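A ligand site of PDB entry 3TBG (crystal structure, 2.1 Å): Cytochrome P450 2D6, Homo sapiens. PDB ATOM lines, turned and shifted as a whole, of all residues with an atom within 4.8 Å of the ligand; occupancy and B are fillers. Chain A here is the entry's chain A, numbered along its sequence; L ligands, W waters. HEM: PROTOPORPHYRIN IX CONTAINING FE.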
ATOM      1  N   LEU A  69     -10.816 -34.743  35.925  1.00  0.00           N
ATOM      2  CA  LEU A  69     -10.368 -34.143  34.666  1.00  0.00           C
ATOM      3  C   LEU A  69      -9.274 -33.080  34.766  1.00  0.00           C
ATOM      4  O   LEU A  69      -8.538 -32.855  33.808  1.00  0.00           O
ATOM      5  CB  LEU A  69     -11.557 -33.542  33.915  1.00  0.00           C
ATOM      6  CG  LEU A  69     -12.740 -34.434  33.500  1.00  0.00           C
ATOM      7  CD1 LEU A  69     -13.708 -33.620  32.654  1.00  0.00           C
ATOM      8  CD2 LEU A  69     -12.263 -35.646  32.739  1.00  0.00           C
ATOM      9  N   ARG A  79      -9.730 -41.777  25.677  1.00  0.00           N
ATOM     10  CA  ARG A  79     -11.083 -42.159  25.288  1.00  0.00           C
ATOM     11  C   ARG A  79     -11.129 -43.682  25.268  1.00  0.00           C
ATOM     12  O   ARG A  79     -10.121 -44.328  24.980  1.00  0.00           O
ATOM     13  CB  ARG A  79     -11.415 -41.686  23.867  1.00  0.00           C
ATOM     14  CG  ARG A  79     -11.406 -40.189  23.622  1.00  0.00           C
ATOM     15  CD  ARG A  79     -12.560 -39.493  24.308  1.00  0.00           C
ATOM     16  NE  ARG A  79     -12.645 -38.088  23.902  1.00  0.00           N
ATOM     17  CZ  ARG A  79     -13.140 -37.128  24.674  1.00  0.00           C
ATOM     18  NH1 ARG A  79     -13.183 -35.872  24.228  1.00  0.00           N
ATOM     19  NH2 ARG A  79     -13.577 -37.416  25.895  1.00  0.00           N
ATOM     20  N   VAL A  97      -9.998 -36.202  16.041  1.00  0.00           N
ATOM     21  CA  VAL A  97      -9.714 -35.540  17.298  1.00  0.00           C
ATOM     22  C   VAL A  97     -10.696 -35.951  18.372  1.00  0.00           C
ATOM     23  O   VAL A  97     -10.298 -36.273  19.492  1.00  0.00           O
ATOM     24  CB  VAL A  97      -9.793 -33.998  17.187  1.00  0.00           C
ATOM     25  CG1 VAL A  97      -9.669 -33.367  18.576  1.00  0.00           C
ATOM     26  CG2 VAL A  97      -8.693 -33.474  16.301  1.00  0.00           C
ATOM     27  N   PHE A  98     -11.976 -35.965  18.022  1.00  0.00           N
ATOM     28  CA  PHE A  98     -13.034 -36.282  18.973  1.00  0.00           C
ATOM     29  C   PHE A  98     -12.840 -37.583  19.749  1.00  0.00           C
ATOM     30  O   PHE A  98     -12.855 -37.559  20.974  1.00  0.00           O
ATOM     31  CB  PHE A  98     -14.379 -36.317  18.240  1.00  0.00           C
ATOM     32  CG  PHE A  98     -15.551 -36.076  19.138  1.00  0.00           C
ATOM     33  CD1 PHE A  98     -15.898 -34.792  19.520  1.00  0.00           C
ATOM     34  CD2 PHE A  98     -16.320 -37.142  19.604  1.00  0.00           C
ATOM     35  CE1 PHE A  98     -17.000 -34.562  20.357  1.00  0.00           C
ATOM     36  CE2 PHE A  98     -17.415 -36.920  20.433  1.00  0.00           C
ATOM     37  CZ  PHE A  98     -17.755 -35.625  20.811  1.00  0.00           C
ATOM     38  N   TRP A 106      -3.648 -37.513  18.638  1.00  0.00           N
ATOM     39  CA  TRP A 106      -4.682 -36.624  19.146  1.00  0.00           C
ATOM     40  C   TRP A 106      -4.124 -35.240  19.407  1.00  0.00           C
ATOM     41  O   TRP A 106      -4.719 -34.238  19.021  1.00  0.00           O
ATOM     42  CB  TRP A 106      -5.258 -37.153  20.458  1.00  0.00           C
ATOM     43  CG  TRP A 106      -6.012 -36.091  21.221  1.00  0.00           C
ATOM     44  CD1 TRP A 106      -7.309 -35.702  21.040  1.00  0.00           C
ATOM     45  CD2 TRP A 106      -5.490 -35.250  22.277  1.00  0.00           C
ATOM     46  NE1 TRP A 106      -7.628 -34.682  21.908  1.00  0.00           N
ATOM     47  CE2 TRP A 106      -6.533 -34.379  22.671  1.00  0.00           C
ATOM     48  CE3 TRP A 106      -4.238 -35.155  22.907  1.00  0.00           C
ATOM     49  CZ2 TRP A 106      -6.375 -33.426  23.681  1.00  0.00           C
ATOM     50  CZ3 TRP A 106      -4.080 -34.202  23.917  1.00  0.00           C
ATOM     51  CH2 TRP A 106      -5.139 -33.345  24.291  1.00  0.00           C
ATOM     52  N   ARG A 110      -5.314 -31.841  17.979  1.00  0.00           N
ATOM     53  CA  ARG A 110      -5.908 -30.944  18.973  1.00  0.00           C
ATOM     54  C   ARG A 110      -5.236 -29.575  18.837  1.00  0.00           C
ATOM     55  O   ARG A 110      -5.908 -28.550  18.697  1.00  0.00           O
ATOM     56  CB  ARG A 110      -5.654 -31.490  20.385  1.00  0.00           C
ATOM     57  CG  ARG A 110      -6.015 -30.540  21.519  1.00  0.00           C
ATOM     58  CD  ARG A 110      -7.519 -30.500  21.763  1.00  0.00           C
ATOM     59  NE  ARG A 110      -7.885 -29.461  22.730  1.00  0.00           N
ATOM     60  CZ  ARG A 110      -9.023 -29.456  23.416  1.00  0.00           C
ATOM     61  NH1 ARG A 110      -9.910 -30.429  23.259  1.00  0.00           N
ATOM     62  NH2 ARG A 110      -9.274 -28.465  24.249  1.00  0.00           N
ATOM     63  N   LEU A 117      -8.313 -22.332  14.753  1.00  0.00           N
ATOM     64  CA  LEU A 117      -9.523 -21.567  15.097  1.00  0.00           C
ATOM     65  C   LEU A 117      -9.117 -20.200  15.621  1.00  0.00           C
ATOM     66  O   LEU A 117      -9.724 -19.184  15.267  1.00  0.00           O
ATOM     67  CB  LEU A 117     -10.337 -22.284  16.196  1.00  0.00           C
ATOM     68  CG  LEU A 117     -11.201 -23.463  15.762  1.00  0.00           C
ATOM     69  CD1 LEU A 117     -11.685 -24.216  16.984  1.00  0.00           C
ATOM     70  CD2 LEU A 117     -12.372 -22.965  14.925  1.00  0.00           C
ATOM     71  N   LEU A 167     -15.730 -22.527   8.154  1.00  0.00           N
ATOM     72  CA  LEU A 167     -14.495 -22.815   8.890  1.00  0.00           C
ATOM     73  C   LEU A 167     -13.626 -23.863   8.222  1.00  0.00           C
ATOM     74  O   LEU A 167     -12.415 -23.703   8.112  1.00  0.00           O
ATOM     75  CB  LEU A 167     -14.824 -23.295  10.310  1.00  0.00           C
ATOM     76  CG  LEU A 167     -13.764 -24.186  10.991  1.00  0.00           C
ATOM     77  CD1 LEU A 167     -12.545 -23.358  11.360  1.00  0.00           C
ATOM     78  CD2 LEU A 167     -14.352 -24.836  12.254  1.00  0.00           C
ATOM     79  N   LEU A 280     -15.506 -32.104  13.325  1.00  0.00           N
ATOM     80  CA  LEU A 280     -15.893 -30.718  13.580  1.00  0.00           C
ATOM     81  C   LEU A 280     -17.370 -30.509  13.248  1.00  0.00           C
ATOM     82  O   LEU A 280     -18.084 -29.817  13.976  1.00  0.00           O
ATOM     83  CB  LEU A 280     -15.007 -29.774  12.760  1.00  0.00           C
ATOM     84  CG  LEU A 280     -13.528 -29.832  13.148  1.00  0.00           C
ATOM     85  CD1 LEU A 280     -12.699 -28.964  12.210  1.00  0.00           C
ATOM     86  CD2 LEU A 280     -13.371 -29.365  14.589  1.00  0.00           C
ATOM     87  N   ALA A 283     -19.454 -32.712  16.046  1.00  0.00           N
ATOM     88  CA  ALA A 283     -19.406 -32.133  17.390  1.00  0.00           C
ATOM     89  C   ALA A 283     -19.923 -30.705  17.469  1.00  0.00           C
ATOM     90  O   ALA A 283     -20.387 -30.276  18.521  1.00  0.00           O
ATOM     91  CB  ALA A 283     -17.984 -32.185  17.925  1.00  0.00           C
ATOM     92  N   GLY A 284     -19.847 -29.973  16.353  1.00  0.00           N
ATOM     93  CA  GLY A 284     -20.262 -28.587  16.357  1.00  0.00           C
ATOM     94  C   GLY A 284     -21.621 -28.194  15.816  1.00  0.00           C
ATOM     95  O   GLY A 284     -22.091 -27.073  16.039  1.00  0.00           O
ATOM     96  N   THR A 287     -24.907 -29.704  18.616  1.00  0.00           N
ATOM     97  CA  THR A 287     -24.762 -29.011  19.891  1.00  0.00           C
ATOM     98  C   THR A 287     -25.211 -27.547  19.814  1.00  0.00           C
ATOM     99  O   THR A 287     -26.138 -27.135  20.501  1.00  0.00           O
ATOM    100  CB  THR A 287     -23.307 -29.025  20.350  1.00  0.00           C
ATOM    101  OG1 THR A 287     -22.465 -28.589  19.278  1.00  0.00           O
ATOM    102  CG2 THR A 287     -22.901 -30.414  20.807  1.00  0.00           C
ATOM    103  N   THR A 288     -24.556 -26.777  18.953  1.00  0.00           N
ATOM    104  CA  THR A 288     -24.868 -25.365  18.792  1.00  0.00           C
ATOM    105  C   THR A 288     -26.310 -25.161  18.320  1.00  0.00           C
ATOM    106  O   THR A 288     -27.010 -24.267  18.804  1.00  0.00           O
ATOM    107  CB  THR A 288     -23.913 -24.726  17.772  1.00  0.00           C
ATOM    108  OG1 THR A 288     -22.568 -25.123  18.077  1.00  0.00           O
ATOM    109  CG2 THR A 288     -23.980 -23.202  17.832  1.00  0.00           C
ATOM    110  N   THR A 291     -28.779 -25.968  21.112  1.00  0.00           N
ATOM    111  CA  THR A 291     -28.716 -24.898  22.115  1.00  0.00           C
ATOM    112  C   THR A 291     -29.563 -23.724  21.651  1.00  0.00           C
ATOM    113  O   THR A 291     -30.379 -23.200  22.418  1.00  0.00           O
ATOM    114  CB  THR A 291     -27.258 -24.453  22.349  1.00  0.00           C
ATOM    115  OG1 THR A 291     -26.497 -25.566  22.849  1.00  0.00           O
ATOM    116  CG2 THR A 291     -27.188 -23.311  23.387  1.00  0.00           C
ATOM    117  N   GLN A 342     -27.885 -22.294  28.088  1.00  0.00           N
ATOM    118  CA  GLN A 342     -26.992 -23.448  28.089  1.00  0.00           C
ATOM    119  C   GLN A 342     -27.106 -24.259  29.388  1.00  0.00           C
ATOM    120  O   GLN A 342     -27.102 -25.496  29.368  1.00  0.00           O
ATOM    121  CB  GLN A 342     -25.548 -23.010  27.910  1.00  0.00           C
ATOM    122  CG  GLN A 342     -25.204 -22.520  26.522  1.00  0.00           C
ATOM    123  CD  GLN A 342     -23.701 -22.425  26.315  1.00  0.00           C
ATOM    124  OE1 GLN A 342     -23.075 -21.417  26.628  1.00  0.00           O
ATOM    125  NE2 GLN A 342     -23.113 -23.507  25.798  1.00  0.00           N
ATOM    126  N   ILE A 347     -27.758 -29.583  27.137  1.00  0.00           N
ATOM    127  CA  ILE A 347     -27.825 -30.422  25.948  1.00  0.00           C
ATOM    128  C   ILE A 347     -26.941 -31.665  25.895  1.00  0.00           C
ATOM    129  O   ILE A 347     -27.262 -32.608  25.168  1.00  0.00           O
ATOM    130  CB  ILE A 347     -27.541 -29.607  24.685  1.00  0.00           C
ATOM    131  CG1 ILE A 347     -26.104 -29.102  24.714  1.00  0.00           C
ATOM    132  CG2 ILE A 347     -28.518 -28.447  24.580  1.00  0.00           C
ATOM    133  CD1 ILE A 347     -25.585 -28.703  23.365  1.00  0.00           C
ATOM    134  N   VAL A 348     -25.839 -31.647  26.630  1.00  0.00           N
ATOM    135  CA  VAL A 348     -24.932 -32.794  26.677  1.00  0.00           C
ATOM    136  C   VAL A 348     -24.804 -33.187  28.144  1.00  0.00           C
ATOM    137  O   VAL A 348     -23.740 -33.054  28.741  1.00  0.00           O
ATOM    138  CB  VAL A 348     -23.523 -32.439  26.136  1.00  0.00           C
ATOM    139  CG1 VAL A 348     -22.721 -33.720  25.915  1.00  0.00           C
ATOM    140  CG2 VAL A 348     -23.626 -31.658  24.837  1.00  0.00           C
ATOM    141  N   GLY A 351     -21.884 -35.571  28.944  1.00  0.00           N
ATOM    142  CA  GLY A 351     -20.650 -35.266  28.236  1.00  0.00           C
ATOM    143  C   GLY A 351     -20.195 -36.345  27.269  1.00  0.00           C
ATOM    144  O   GLY A 351     -20.995 -37.031  26.651  1.00  0.00           O
ATOM    145  N   VAL A 352     -18.879 -36.476  27.118  1.00  0.00           N
ATOM    146  CA  VAL A 352     -18.305 -37.503  26.256  1.00  0.00           C
ATOM    147  C   VAL A 352     -17.423 -38.321  27.187  1.00  0.00           C
ATOM    148  O   VAL A 352     -16.686 -37.750  28.013  1.00  0.00           O
ATOM    149  CB  VAL A 352     -17.464 -36.870  25.114  1.00  0.00           C
ATOM    150  CG1 VAL A 352     -16.825 -37.955  24.252  1.00  0.00           C
ATOM    151  CG2 VAL A 352     -18.376 -35.994  24.250  1.00  0.00           C
ATOM    152  N   HIS A 354     -14.571 -40.578  29.011  1.00  0.00           N
ATOM    153  CA  HIS A 354     -13.119 -40.550  29.137  1.00  0.00           C
ATOM    154  C   HIS A 354     -12.727 -41.938  29.667  1.00  0.00           C
ATOM    155  O   HIS A 354     -13.589 -42.731  30.052  1.00  0.00           O
ATOM    156  CB  HIS A 354     -12.655 -39.527  30.161  1.00  0.00           C
ATOM    157  CG  HIS A 354     -12.838 -38.108  29.741  1.00  0.00           C
ATOM    158  ND1 HIS A 354     -11.784 -37.242  29.587  1.00  0.00           N
ATOM    159  CD2 HIS A 354     -13.959 -37.388  29.510  1.00  0.00           C
ATOM    160  CE1 HIS A 354     -12.238 -36.043  29.267  1.00  0.00           C
ATOM    161  NE2 HIS A 354     -13.559 -36.105  29.217  1.00  0.00           N
ATOM    162  N   LEU A 377     -22.222 -33.881  33.498  1.00  0.00           N
ATOM    163  CA  LEU A 377     -22.188 -32.422  33.419  1.00  0.00           C
ATOM    164  C   LEU A 377     -23.488 -31.833  33.903  1.00  0.00           C
ATOM    165  O   LEU A 377     -23.534 -30.724  34.429  1.00  0.00           O
ATOM    166  CB  LEU A 377     -21.912 -31.974  31.981  1.00  0.00           C
ATOM    167  CG  LEU A 377     -20.553 -32.459  31.476  1.00  0.00           C
ATOM    168  CD1 LEU A 377     -20.303 -31.983  30.060  1.00  0.00           C
ATOM    169  CD2 LEU A 377     -19.481 -31.953  32.413  1.00  0.00           C
ATOM    170  N   PRO A 413     -20.641 -26.505  30.738  1.00  0.00           N
ATOM    171  CA  PRO A 413     -21.290 -27.266  29.663  1.00  0.00           C
ATOM    172  C   PRO A 413     -20.297 -27.801  28.613  1.00  0.00           C
ATOM    173  O   PRO A 413     -20.666 -28.665  27.804  1.00  0.00           O
ATOM    174  CB  PRO A 413     -22.243 -26.230  29.063  1.00  0.00           C
ATOM    175  CG  PRO A 413     -21.424 -24.939  29.188  1.00  0.00           C
ATOM    176  CD  PRO A 413     -20.878 -25.056  30.604  1.00  0.00           C
ATOM    177  N   PHE A 414     -19.060 -27.305  28.634  1.00  0.00           N
ATOM    178  CA  PHE A 414     -18.050 -27.739  27.663  1.00  0.00           C
ATOM    179  C   PHE A 414     -17.058 -28.671  28.323  1.00  0.00           C
ATOM    180  O   PHE A 414     -16.014 -28.979  27.748  1.00  0.00           O
ATOM    181  CB  PHE A 414     -17.281 -26.542  27.100  1.00  0.00           C
ATOM    182  CG  PHE A 414     -18.148 -25.500  26.445  1.00  0.00           C
ATOM    183  CD1 PHE A 414     -18.494 -24.333  27.133  1.00  0.00           C
ATOM    184  CD2 PHE A 414     -18.624 -25.672  25.143  1.00  0.00           C
ATOM    185  CE1 PHE A 414     -19.295 -23.342  26.524  1.00  0.00           C
ATOM    186  CE2 PHE A 414     -19.428 -24.700  24.529  1.00  0.00           C
ATOM    187  CZ  PHE A 414     -19.759 -23.534  25.216  1.00  0.00           C
ATOM    188  N   SER A 415     -17.380 -29.088  29.556  1.00  0.00           N
ATOM    189  CA  SER A 415     -16.534 -29.979  30.348  1.00  0.00           C
ATOM    190  C   SER A 415     -15.282 -29.250  30.837  1.00  0.00           C
ATOM    191  O   SER A 415     -15.264 -28.019  30.907  1.00  0.00           O
ATOM    192  CB  SER A 415     -16.153 -31.229  29.536  1.00  0.00           C
ATOM    193  OG  SER A 415     -15.572 -32.217  30.395  1.00  0.00           O
ATOM    194  N   ALA A 416     -14.235 -30.002  31.174  1.00  0.00           N
ATOM    195  CA  ALA A 416     -12.993 -29.435  31.685  1.00  0.00           C
ATOM    196  C   ALA A 416     -11.793 -30.304  31.341  1.00  0.00           C
ATOM    197  O   ALA A 416     -11.949 -31.439  30.904  1.00  0.00           O
ATOM    198  CB  ALA A 416     -13.071 -29.263  33.220  1.00  0.00           C
ATOM    199  N   ARG A 418      -7.867 -31.236  29.579  1.00  0.00           N
ATOM    200  CA  ARG A 418      -7.253 -31.375  28.253  1.00  0.00           C
ATOM    201  C   ARG A 418      -8.185 -31.699  27.100  1.00  0.00           C
ATOM    202  O   ARG A 418      -7.880 -31.376  25.950  1.00  0.00           O
ATOM    203  CB  ARG A 418      -6.192 -32.489  28.277  1.00  0.00           C
ATOM    204  CG  ARG A 418      -4.985 -32.263  29.162  1.00  0.00           C
ATOM    205  CD  ARG A 418      -4.275 -33.611  29.361  1.00  0.00           C
ATOM    206  NE  ARG A 418      -2.891 -33.476  29.800  1.00  0.00           N
ATOM    207  CZ  ARG A 418      -2.526 -32.926  30.947  1.00  0.00           C
ATOM    208  NH1 ARG A 418      -1.234 -32.861  31.261  1.00  0.00           N
ATOM    209  NH2 ARG A 418      -3.432 -32.445  31.787  1.00  0.00           N
ATOM    210  N   ARG A 419      -9.318 -32.354  27.383  1.00  0.00           N
ATOM    211  CA  ARG A 419     -10.256 -32.733  26.317  1.00  0.00           C
ATOM    212  C   ARG A 419     -11.487 -31.832  26.221  1.00  0.00           C
ATOM    213  O   ARG A 419     -12.384 -32.079  25.414  1.00  0.00           O
ATOM    214  CB  ARG A 419     -10.701 -34.185  26.518  1.00  0.00           C
ATOM    215  CG  ARG A 419      -9.629 -35.189  26.221  1.00  0.00           C
ATOM    216  CD  ARG A 419      -9.451 -35.366  24.702  1.00  0.00           C
ATOM    217  NE  ARG A 419      -8.653 -36.542  24.481  1.00  0.00           N
ATOM    218  CZ  ARG A 419      -8.811 -37.433  23.510  1.00  0.00           C
ATOM    219  NH1 ARG A 419      -9.776 -37.295  22.579  1.00  0.00           N
ATOM    220  NH2 ARG A 419      -8.014 -38.480  23.501  1.00  0.00           N
ATOM    221  N   ALA A 420     -11.526 -30.788  27.053  1.00  0.00           N
ATOM    222  CA  ALA A 420     -12.640 -29.854  27.058  1.00  0.00           C
ATOM    223  C   ALA A 420     -12.906 -29.356  25.638  1.00  0.00           C
ATOM    224  O   ALA A 420     -11.981 -29.224  24.837  1.00  0.00           O
ATOM    225  CB  ALA A 420     -12.309 -28.665  27.984  1.00  0.00           C
ATOM    226  N   CYS A 421     -14.170 -29.073  25.341  1.00  0.00           N
ATOM    227  CA  CYS A 421     -14.554 -28.610  24.011  1.00  0.00           C
ATOM    228  C   CYS A 421     -13.559 -27.638  23.386  1.00  0.00           C
ATOM    229  O   CYS A 421     -13.289 -26.570  23.947  1.00  0.00           O
ATOM    230  CB  CYS A 421     -15.929 -27.938  24.075  1.00  0.00           C
ATOM    231  SG  CYS A 421     -16.587 -27.450  22.458  1.00  0.00           S
ATOM    232  N   LEU A 422     -13.002 -27.994  22.225  1.00  0.00           N
ATOM    233  CA  LEU A 422     -12.085 -27.083  21.551  1.00  0.00           C
ATOM    234  C   LEU A 422     -12.877 -26.082  20.718  1.00  0.00           C
ATOM    235  O   LEU A 422     -12.351 -25.104  20.242  1.00  0.00           O
ATOM    236  CB  LEU A 422     -11.086 -27.845  20.673  1.00  0.00           C
ATOM    237  CG  LEU A 422     -11.557 -28.736  19.516  1.00  0.00           C
ATOM    238  CD1 LEU A 422     -12.003 -27.897  18.319  1.00  0.00           C
ATOM    239  CD2 LEU A 422     -10.403 -29.641  19.132  1.00  0.00           C
ATOM    240  N   GLY A 423     -14.174 -26.329  20.574  1.00  0.00           N
ATOM    241  CA  GLY A 423     -14.982 -25.405  19.800  1.00  0.00           C
ATOM    242  C   GLY A 423     -15.627 -24.320  20.624  1.00  0.00           C
ATOM    243  O   GLY A 423     -16.336 -23.469  20.075  1.00  0.00           O
ATOM    244  N   LEU A 426     -15.705 -20.678  19.348  1.00  0.00           N
ATOM    245  CA  LEU A 426     -16.597 -20.529  18.202  1.00  0.00           C
ATOM    246  C   LEU A 426     -18.054 -20.659  18.629  1.00  0.00           C
ATOM    247  O   LEU A 426     -18.916 -19.911  18.164  1.00  0.00           O
ATOM    248  CB  LEU A 426     -16.265 -21.565  17.125  1.00  0.00           C
ATOM    249  CG  LEU A 426     -17.138 -21.584  15.868  1.00  0.00           C
ATOM    250  CD1 LEU A 426     -17.169 -20.214  15.233  1.00  0.00           C
ATOM    251  CD2 LEU A 426     -16.592 -22.602  14.875  1.00  0.00           C
ATOM    252  N   ALA A 427     -18.338 -21.619  19.514  1.00  0.00           N
ATOM    253  CA  ALA A 427     -19.701 -21.807  20.000  1.00  0.00           C
ATOM    254  C   ALA A 427     -20.191 -20.517  20.673  1.00  0.00           C
ATOM    255  O   ALA A 427     -21.321 -20.097  20.469  1.00  0.00           O
ATOM    256  CB  ALA A 427     -19.742 -22.971  21.005  1.00  0.00           C
ATOM    257  N   GLU A 430     -21.034 -18.015  17.928  1.00  0.00           N
ATOM    258  CA  GLU A 430     -22.277 -18.382  17.260  1.00  0.00           C
ATOM    259  C   GLU A 430     -23.504 -18.127  18.130  1.00  0.00           C
ATOM    260  O   GLU A 430     -24.499 -17.574  17.666  1.00  0.00           O
ATOM    261  CB  GLU A 430     -22.270 -19.868  16.863  1.00  0.00           C
ATOM    262  CG  GLU A 430     -21.288 -20.238  15.785  1.00  0.00           C
ATOM    263  CD  GLU A 430     -21.496 -21.675  15.329  1.00  0.00           C
ATOM    264  OE1 GLU A 430     -22.480 -21.940  14.616  1.00  0.00           O
ATOM    265  OE2 GLU A 430     -20.688 -22.536  15.731  1.00  0.00           O
ATOM    266  N   LEU A 431     -23.450 -18.540  19.397  1.00  0.00           N
ATOM    267  CA  LEU A 431     -24.589 -18.329  20.280  1.00  0.00           C
ATOM    268  C   LEU A 431     -24.915 -16.839  20.441  1.00  0.00           C
ATOM    269  O   LEU A 431     -26.076 -16.440  20.362  1.00  0.00           O
ATOM    270  CB  LEU A 431     -24.342 -18.948  21.658  1.00  0.00           C
ATOM    271  CG  LEU A 431     -24.262 -20.484  21.711  1.00  0.00           C
ATOM    272  CD1 LEU A 431     -24.160 -20.920  23.157  1.00  0.00           C
ATOM    273  CD2 LEU A 431     -25.501 -21.087  21.066  1.00  0.00           C
HETATM  274  CHA HEM L   1     -15.815 -31.846  22.827  1.00  0.00           C
HETATM  275  CHB HEM L   1     -19.746 -29.558  24.259  1.00  0.00           C
HETATM  276  CHC HEM L   1     -19.710 -27.037  20.276  1.00  0.00           C
HETATM  277  CHD HEM L   1     -15.811 -29.289  18.874  1.00  0.00           C
HETATM  278  C1A HEM L   1     -16.934 -31.498  23.624  1.00  0.00           C
HETATM  279  C2A HEM L   1     -17.299 -32.058  24.859  1.00  0.00           C
HETATM  280  C3A HEM L   1     -18.425 -31.380  25.263  1.00  0.00           C
HETATM  281  C4A HEM L   1     -18.683 -30.439  24.268  1.00  0.00           C
HETATM  282  CMA HEM L   1     -19.254 -31.607  26.591  1.00  0.00           C
HETATM  283  CAA HEM L   1     -16.576 -33.194  25.565  1.00  0.00           C
HETATM  284  CBA HEM L   1     -15.484 -32.770  26.493  1.00  0.00           C
HETATM  285  CGA HEM L   1     -14.815 -33.942  27.195  1.00  0.00           C
HETATM  286  O1A HEM L   1     -14.376 -34.897  26.540  1.00  0.00           O
HETATM  287  O2A HEM L   1     -14.742 -33.968  28.416  1.00  0.00           O
HETATM  288  C1B HEM L   1     -20.185 -28.651  23.301  1.00  0.00           C
HETATM  289  C2B HEM L   1     -21.266 -27.737  23.441  1.00  0.00           C
HETATM  290  C3B HEM L   1     -21.221 -26.961  22.255  1.00  0.00           C
HETATM  291  C4B HEM L   1     -20.119 -27.473  21.530  1.00  0.00           C
HETATM  292  CMB HEM L   1     -22.223 -27.681  24.624  1.00  0.00           C
HETATM  293  CAB HEM L   1     -22.047 -25.868  21.814  1.00  0.00           C
HETATM  294  CBB HEM L   1     -23.172 -25.168  22.473  1.00  0.00           C
HETATM  295  C1C HEM L   1     -18.579 -27.328  19.532  1.00  0.00           C
HETATM  296  C2C HEM L   1     -18.270 -26.757  18.312  1.00  0.00           C
HETATM  297  C3C HEM L   1     -17.198 -27.488  17.783  1.00  0.00           C
HETATM  298  C4C HEM L   1     -16.930 -28.478  18.764  1.00  0.00           C
HETATM  299  CMC HEM L   1     -19.011 -25.530  17.661  1.00  0.00           C
HETATM  300  CAC HEM L   1     -16.488 -27.388  16.613  1.00  0.00           C
HETATM  301  CBC HEM L   1     -15.836 -26.287  16.028  1.00  0.00           C
HETATM  302  C1D HEM L   1     -15.538 -30.290  19.743  1.00  0.00           C
HETATM  303  C2D HEM L   1     -14.502 -31.232  19.609  1.00  0.00           C
HETATM  304  C3D HEM L   1     -14.425 -31.916  20.794  1.00  0.00           C
HETATM  305  C4D HEM L   1     -15.423 -31.362  21.593  1.00  0.00           C
HETATM  306  CMD HEM L   1     -13.594 -31.487  18.369  1.00  0.00           C
HETATM  307  CAD HEM L   1     -13.453 -33.059  21.175  1.00  0.00           C
HETATM  308  CBD HEM L   1     -12.166 -32.469  21.811  1.00  0.00           C
HETATM  309  CGD HEM L   1     -11.072 -33.450  22.277  1.00  0.00           C
HETATM  310  O1D HEM L   1      -9.967 -33.055  22.522  1.00  0.00           O
HETATM  311  O2D HEM L   1     -11.358 -34.660  22.380  1.00  0.00           O
HETATM  312  NA  HEM L   1     -17.799 -30.507  23.299  1.00  0.00           N
HETATM  313  NB  HEM L   1     -19.532 -28.470  22.160  1.00  0.00           N
HETATM  314  NC  HEM L   1     -17.786 -28.339  19.804  1.00  0.00           N
HETATM  315  ND  HEM L   1     -16.055 -30.392  20.925  1.00  0.00           N
HETATM  316 FE   HEM L   1     -17.750 -29.352  21.580  1.00  0.00          FE
HETATM  317  O   HOH W   1     -19.175 -31.516  20.952  1.00  0.00           O
HETATM  318  O   HOH W   2     -17.510 -34.692  28.975  1.00  0.00           O
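The indole nitrogen (NE1) of Trp 106 is in hydrogen-bond range of an oxygen (O1D) of the ligand, at 2.9 Å. OG of Ser 415 lies within hydrogen-bond range of O2A of the ligand (2.8 Å). An iron atom (FE) of the ligand is bound by the side-chain sulfur (SG) of Cys 421 (2.4 Å). An oxygen (O2A) of the ligand sits at hydrogen-bond distance from a ring nitrogen (NE2) of His 354, 2.6 Å away. The guanidinium group (NH1) of Arg 419 is in salt-bridge range of an oxygen (O2D) of the ligand (3.1 Å). The guanidinium group (NH1) of Arg 110 lies within salt-bridge range of an oxygen (O1D) of the ligand (2.7 Å). O1A of the ligand is in salt-bridge range of NH2 of Arg 79 (2.7 Å).
The backbone carbonyl oxygen (O) of Phe 98 lies within hydrogen-bond range of the guanidinium group (NE) of Arg 79 (3.0 Å). The backbone carbonyl oxygen (O) of Ala 283 sits at hydrogen-bond distance from the side-chain hydroxyl (OG1) of Thr 287, at 2.8 Å. The backbone carbonyl oxygen of Gly 284 lies within hydrogen-bond range of the side-chain hydroxyl of Thr 288, at 2.9 Å. The backbone carbonyl oxygen (O) of Phe 414 sits at hydrogen-bond distance from the backbone NH (N) of Cys 421 (3.0 Å). The guanidinium group (NH1) of Arg 419 sits at hydrogen-bond distance from the backbone carbonyl oxygen (O) of Phe 98. NH1 of Arg 110 is in hydrogen-bond range of O of Ala 420 (2.9 Å). O of Val 97 sits at hydrogen-bond distance from NH1 of Arg 419, at 3.3 Å. O of Thr 287 sits at hydrogen-bond distance from OG1 of Thr 291 (2.8 Å).
The backbone carbonyl oxygen (O) of Val 97 lies close to an oxygen (O2D) of the ligand, 3.5 Å away. The backbone carbonyl oxygen (O) of Ala 283 sits close to a nitrogen (NC) of the ligand, at 3.5 Å. Phe 98 touches the ligand (CD1 to CAD, 3.4 Å). Leu 280 touches the ligand (O to CAC, 3.9 Å). CA of Gly 284 touches C2C of the ligand, at 3.3 Å. Thr 287 touches the ligand. Thr 288 touches the ligand. Thr 291 touches the ligand (OG1 to CBB, 3.4 Å). NE2 of Gln 342 touches CBB of the ligand, 3.7 Å away. CD1 of Ile 347 touches CMB of the ligand (3.7 Å). Val 352 touches the ligand (CG2 to CAA, 3.6 Å). Leu 377 touches the ligand (CD1 to CMA, 3.6 Å). O of Pro 413 touches CMA of the ligand, at 3.5 Å. Phe 414 touches the ligand. CG of Leu 422 touches CMD of the ligand (3.6 Å). Gly 423 touches the ligand. CD2 of Leu 426 touches CBC of the ligand (3.9 Å). Ala 427 touches the ligand (CB to CAB, 3.8 Å). Glu 430 touches the ligand. Along chain A the residues within 4 Å of the ligand span positions 79 to 430.
Water W2 lies within hydrogen-bond range of O2A of the ligand (2.9 Å), N of Val 352 (2.9 Å) and OG of Ser 415 (3.4 Å).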
